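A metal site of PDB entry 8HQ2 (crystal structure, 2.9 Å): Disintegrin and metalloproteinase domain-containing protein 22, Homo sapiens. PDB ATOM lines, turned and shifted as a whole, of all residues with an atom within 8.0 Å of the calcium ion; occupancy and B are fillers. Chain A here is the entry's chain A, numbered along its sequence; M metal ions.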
ATOM      1  N   SER A 207       6.796   6.117 -24.805  1.00  0.00           N
ATOM      2  CA  SER A 207       5.430   5.921 -24.342  1.00  0.00           C
ATOM      3  C   SER A 207       5.003   6.991 -23.339  1.00  0.00           C
ATOM      4  O   SER A 207       3.876   7.496 -23.396  1.00  0.00           O
ATOM      5  CB  SER A 207       5.272   4.527 -23.734  1.00  0.00           C
ATOM      6  OG  SER A 207       6.268   4.278 -22.753  1.00  0.00           O
ATOM      7  N   LEU A 209       6.054  10.626 -21.041  1.00  0.00           N
ATOM      8  CA  LEU A 209       6.869  11.837 -21.050  1.00  0.00           C
ATOM      9  C   LEU A 209       6.687  12.573 -19.726  1.00  0.00           C
ATOM     10  O   LEU A 209       5.668  12.436 -19.044  1.00  0.00           O
ATOM     11  CB  LEU A 209       6.501  12.762 -22.225  1.00  0.00           C
ATOM     12  CG  LEU A 209       6.673  12.251 -23.668  1.00  0.00           C
ATOM     13  CD1 LEU A 209       5.587  11.263 -24.075  1.00  0.00           C
ATOM     14  CD2 LEU A 209       6.697  13.425 -24.625  1.00  0.00           C
ATOM     15  N   PRO A 212       3.132  17.145 -18.687  1.00  0.00           N
ATOM     16  CA  PRO A 212       1.759  16.640 -18.667  1.00  0.00           C
ATOM     17  C   PRO A 212       1.285  16.326 -20.075  1.00  0.00           C
ATOM     18  O   PRO A 212       1.594  17.063 -21.030  1.00  0.00           O
ATOM     19  CB  PRO A 212       0.962  17.802 -18.059  1.00  0.00           C
ATOM     20  CG  PRO A 212       1.854  18.999 -18.190  1.00  0.00           C
ATOM     21  CD  PRO A 212       3.240  18.471 -18.057  1.00  0.00           C
ATOM     22  N   PRO A 213       0.544  15.229 -20.250  1.00  0.00           N
ATOM     23  CA  PRO A 213       0.158  14.818 -21.606  1.00  0.00           C
ATOM     24  C   PRO A 213      -0.710  15.861 -22.299  1.00  0.00           C
ATOM     25  O   PRO A 213      -1.639  16.402 -21.704  1.00  0.00           O
ATOM     26  CB  PRO A 213      -0.614  13.511 -21.368  1.00  0.00           C
ATOM     27  CG  PRO A 213      -1.024  13.561 -19.921  1.00  0.00           C
ATOM     28  CD  PRO A 213       0.070  14.307 -19.222  1.00  0.00           C
ATOM     29  N   GLU A 214      -0.380  16.130 -23.553  1.00  0.00           N
ATOM     30  CA  GLU A 214      -1.169  16.995 -24.415  1.00  0.00           C
ATOM     31  C   GLU A 214      -1.537  16.225 -25.672  1.00  0.00           C
ATOM     32  O   GLU A 214      -0.745  15.405 -26.173  1.00  0.00           O
ATOM     33  CB  GLU A 214      -0.407  18.283 -24.782  1.00  0.00           C
ATOM     34  CG  GLU A 214       0.667  18.109 -25.845  1.00  0.00           C
ATOM     35  CD  GLU A 214       1.365  19.410 -26.212  1.00  0.00           C
ATOM     36  OE1 GLU A 214       0.674  20.323 -26.718  1.00  0.00           O
ATOM     37  OE2 GLU A 214       2.593  19.511 -26.006  1.00  0.00           O
ATOM     38  N   CYS A 215      -2.738  16.457 -26.179  1.00  0.00           N
ATOM     39  CA  CYS A 215      -3.171  15.788 -27.401  1.00  0.00           C
ATOM     40  C   CYS A 215      -2.604  16.505 -28.620  1.00  0.00           C
ATOM     41  O   CYS A 215      -2.518  17.731 -28.660  1.00  0.00           O
ATOM     42  CB  CYS A 215      -4.687  15.735 -27.489  1.00  0.00           C
ATOM     43  SG  CYS A 215      -5.230  14.904 -28.995  1.00  0.00           S
ATOM     44  N   GLY A 216      -2.231  15.713 -29.617  1.00  0.00           N
ATOM     45  CA  GLY A 216      -1.698  16.249 -30.852  1.00  0.00           C
ATOM     46  C   GLY A 216      -0.211  16.485 -30.884  1.00  0.00           C
ATOM     47  O   GLY A 216       0.272  17.144 -31.819  1.00  0.00           O
ATOM     48  N   ASN A 217       0.546  15.992 -29.905  1.00  0.00           N
ATOM     49  CA  ASN A 217       1.985  16.163 -29.875  1.00  0.00           C
ATOM     50  C   ASN A 217       2.725  15.087 -30.644  1.00  0.00           C
ATOM     51  O   ASN A 217       3.950  15.191 -30.809  1.00  0.00           O
ATOM     52  CB  ASN A 217       2.492  16.208 -28.432  1.00  0.00           C
ATOM     53  CG  ASN A 217       2.230  14.920 -27.683  1.00  0.00           C
ATOM     54  OD1 ASN A 217       1.321  14.165 -28.029  1.00  0.00           O
ATOM     55  ND2 ASN A 217       3.029  14.653 -26.659  1.00  0.00           N
ATOM     56  N   GLY A 218       2.030  14.056 -31.129  1.00  0.00           N
ATOM     57  CA  GLY A 218       2.640  12.990 -31.890  1.00  0.00           C
ATOM     58  C   GLY A 218       3.089  11.787 -31.096  1.00  0.00           C
ATOM     59  O   GLY A 218       3.452  10.764 -31.690  1.00  0.00           O
ATOM     60  N   PHE A 219       3.046  11.852 -29.764  1.00  0.00           N
ATOM     61  CA  PHE A 219       3.414  10.738 -28.898  1.00  0.00           C
ATOM     62  C   PHE A 219       2.195  10.310 -28.105  1.00  0.00           C
ATOM     63  O   PHE A 219       1.523  11.147 -27.486  1.00  0.00           O
ATOM     64  CB  PHE A 219       4.553  11.131 -27.950  1.00  0.00           C
ATOM     65  CG  PHE A 219       5.800  11.581 -28.641  1.00  0.00           C
ATOM     66  CD1 PHE A 219       6.367  10.817 -29.650  1.00  0.00           C
ATOM     67  CD2 PHE A 219       6.402  12.782 -28.290  1.00  0.00           C
ATOM     68  CE1 PHE A 219       7.514  11.237 -30.282  1.00  0.00           C
ATOM     69  CE2 PHE A 219       7.559  13.210 -28.930  1.00  0.00           C
ATOM     70  CZ  PHE A 219       8.122  12.430 -29.931  1.00  0.00           C
ATOM     71  N   ILE A 220       1.895   9.014 -28.127  1.00  0.00           N
ATOM     72  CA  ILE A 220       0.800   8.505 -27.313  1.00  0.00           C
ATOM     73  C   ILE A 220       1.199   8.578 -25.845  1.00  0.00           C
ATOM     74  O   ILE A 220       2.372   8.402 -25.478  1.00  0.00           O
ATOM     75  CB  ILE A 220       0.413   7.067 -27.735  1.00  0.00           C
ATOM     76  CG1 ILE A 220       1.089   6.021 -26.852  1.00  0.00           C
ATOM     77  CG2 ILE A 220       0.747   6.840 -29.204  1.00  0.00           C
ATOM     78  CD1 ILE A 220       0.160   5.374 -25.834  1.00  0.00           C
ATOM     79  N   GLU A 221       0.205   8.909 -25.019  1.00  0.00           N
ATOM     80  CA  GLU A 221       0.402   9.050 -23.547  1.00  0.00           C
ATOM     81  C   GLU A 221      -0.741   8.311 -22.832  1.00  0.00           C
ATOM     82  O   GLU A 221      -1.781   8.071 -23.479  1.00  0.00           O
ATOM     83  CB  GLU A 221       0.450  10.523 -23.142  1.00  0.00           C
ATOM     84  CG  GLU A 221       1.843  11.122 -23.215  1.00  0.00           C
ATOM     85  CD  GLU A 221       1.933  12.450 -23.938  1.00  0.00           C
ATOM     86  OE1 GLU A 221       3.044  13.001 -24.041  1.00  0.00           O
ATOM     87  OE2 GLU A 221       0.879  12.941 -24.396  1.00  0.00           O
ATOM     88  N   THR A 222      -0.543   7.929 -21.579  1.00  0.00           N
ATOM     89  CA  THR A 222      -1.552   7.195 -20.838  1.00  0.00           C
ATOM     90  C   THR A 222      -2.894   7.938 -20.907  1.00  0.00           C
ATOM     91  O   THR A 222      -2.952   9.161 -20.738  1.00  0.00           O
ATOM     92  CB  THR A 222      -1.122   6.972 -19.392  1.00  0.00           C
ATOM     93  OG1 THR A 222      -2.150   6.274 -18.680  1.00  0.00           O
ATOM     94  CG2 THR A 222      -0.815   8.304 -18.694  1.00  0.00           C
ATOM     95  N   GLU A 224      -4.469   8.230 -23.701  1.00  0.00           N
ATOM     96  CA  GLU A 224      -4.594   8.584 -25.109  1.00  0.00           C
ATOM     97  C   GLU A 224      -4.712   7.316 -25.937  1.00  0.00           C
ATOM     98  O   GLU A 224      -3.772   6.507 -25.975  1.00  0.00           O
ATOM     99  CB  GLU A 224      -3.407   9.419 -25.584  1.00  0.00           C
ATOM    100  CG  GLU A 224      -3.408  10.852 -25.132  1.00  0.00           C
ATOM    101  CD  GLU A 224      -2.204  11.599 -25.649  1.00  0.00           C
ATOM    102  OE1 GLU A 224      -1.282  10.936 -26.162  1.00  0.00           O
ATOM    103  OE2 GLU A 224      -2.187  12.845 -25.565  1.00  0.00           O
ATOM    104  N   GLU A 225      -5.871   7.121 -26.578  1.00  0.00           N
ATOM    105  CA  GLU A 225      -6.035   5.984 -27.466  1.00  0.00           C
ATOM    106  C   GLU A 225      -5.094   6.064 -28.667  1.00  0.00           C
ATOM    107  O   GLU A 225      -4.559   5.049 -29.114  1.00  0.00           O
ATOM    108  CB  GLU A 225      -7.494   5.891 -27.920  1.00  0.00           C
ATOM    109  CG  GLU A 225      -8.445   5.367 -26.855  1.00  0.00           C
ATOM    110  CD  GLU A 225      -9.895   5.615 -27.200  1.00  0.00           C
ATOM    111  OE1 GLU A 225     -10.163   6.374 -28.146  1.00  0.00           O
ATOM    112  OE2 GLU A 225     -10.779   5.047 -26.522  1.00  0.00           O
ATOM    113  N   CYS A 226      -4.881   7.271 -29.181  1.00  0.00           N
ATOM    114  CA  CYS A 226      -4.026   7.461 -30.350  1.00  0.00           C
ATOM    115  C   CYS A 226      -3.547   8.902 -30.384  1.00  0.00           C
ATOM    116  O   CYS A 226      -4.139   9.792 -29.772  1.00  0.00           O
ATOM    117  CB  CYS A 226      -4.778   7.114 -31.630  1.00  0.00           C
ATOM    118  SG  CYS A 226      -6.389   7.923 -31.811  1.00  0.00           S
ATOM    119  N   ASP A 227      -2.447   9.118 -31.100  1.00  0.00           N
ATOM    120  CA  ASP A 227      -1.979  10.476 -31.387  1.00  0.00           C
ATOM    121  C   ASP A 227      -1.476  10.540 -32.829  1.00  0.00           C
ATOM    122  O   ASP A 227      -0.521   9.850 -33.174  1.00  0.00           O
ATOM    123  CB  ASP A 227      -0.876  10.892 -30.422  1.00  0.00           C
ATOM    124  CG  ASP A 227      -0.747  12.396 -30.305  1.00  0.00           C
ATOM    125  OD1 ASP A 227      -0.646  13.069 -31.361  1.00  0.00           O
ATOM    126  OD2 ASP A 227      -0.758  12.913 -29.171  1.00  0.00           O
ATOM    127  N   CYS A 228      -2.118  11.368 -33.648  1.00  0.00           N
ATOM    128  CA  CYS A 228      -1.673  11.577 -35.025  1.00  0.00           C
ATOM    129  C   CYS A 228      -0.812  12.815 -35.206  1.00  0.00           C
ATOM    130  O   CYS A 228      -0.296  13.039 -36.309  1.00  0.00           O
ATOM    131  CB  CYS A 228      -2.885  11.664 -35.960  1.00  0.00           C
ATOM    132  SG  CYS A 228      -3.903  13.141 -35.744  1.00  0.00           S
ATOM    133  N   GLY A 229      -0.626  13.632 -34.161  1.00  0.00           N
ATOM    134  CA  GLY A 229       0.181  14.825 -34.267  1.00  0.00           C
ATOM    135  C   GLY A 229      -0.546  16.069 -34.746  1.00  0.00           C
ATOM    136  O   GLY A 229      -1.756  16.209 -34.538  1.00  0.00           O
ATOM    137  N   CYS A 245      -7.254  12.630 -30.222  1.00  0.00           N
ATOM    138  CA  CYS A 245      -6.673  11.521 -29.460  1.00  0.00           C
ATOM    139  C   CYS A 245      -7.725  10.512 -29.009  1.00  0.00           C
ATOM    140  O   CYS A 245      -7.595   9.897 -27.952  1.00  0.00           O
ATOM    141  CB  CYS A 245      -5.863  12.032 -28.276  1.00  0.00           C
ATOM    142  SG  CYS A 245      -4.461  13.041 -28.785  1.00  0.00           S
HETATM  143 CA    CA M   1      -0.305  12.752 -27.123  1.00  0.00          CA
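The side-chain amide nitrogen (ND2) of Asn 217 is in hydrogen-bond range of the side-chain carboxylate (OE1) of Glu 221 (3.1 Å).
The side-chain sulfur (SG) of Cys 215 forms a disulfide with the side-chain sulfur (SG) of Cys 245.
The backbone NH (N) of Gly 216 sits close to the side-chain carboxylate (OD2) of Asp 227, 3.2 Å away.
OD1 of Asp 227 lies within hydrogen-bond range of N of Gly 218 (2.9 Å).
OD1 of Asp 227 is in hydrogen-bond range of N of Gly 229 (2.9 Å).
The side-chain carboxylate (OE1) of Glu 224 sits close to the backbone NH (N) of Glu 221, at 2.8 Å.
The calcium ion is bound by the side-chain carboxylate (OD2) of Asp 227 (2.1 Å), the side-chain carboxylate (OE1) of Glu 224 (2.3 Å), the side-chain amide oxygen (OD1) of Asn 217 (2.3 Å), the side-chain carboxylate (OE2) of Glu 224 (2.4 Å), the backbone carbonyl oxygen (O) of Phe 219 (2.5 Å) and the backbone carbonyl oxygen (O) of Glu 214 (2.9 Å).
The calcium ion has six donor atoms within binding distance.
Slightly farther from the calcium ion lies OE2 of Glu 221 (3.0 Å).
Six residues have an atom within 4 Å of the calcium ion: Glu 214, Asn 217, Phe 219, Glu 221, Glu 224 and Asp 227.
The nearest printed residue that does not touch the calcium ion is Cys 215 (4.2 Å).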
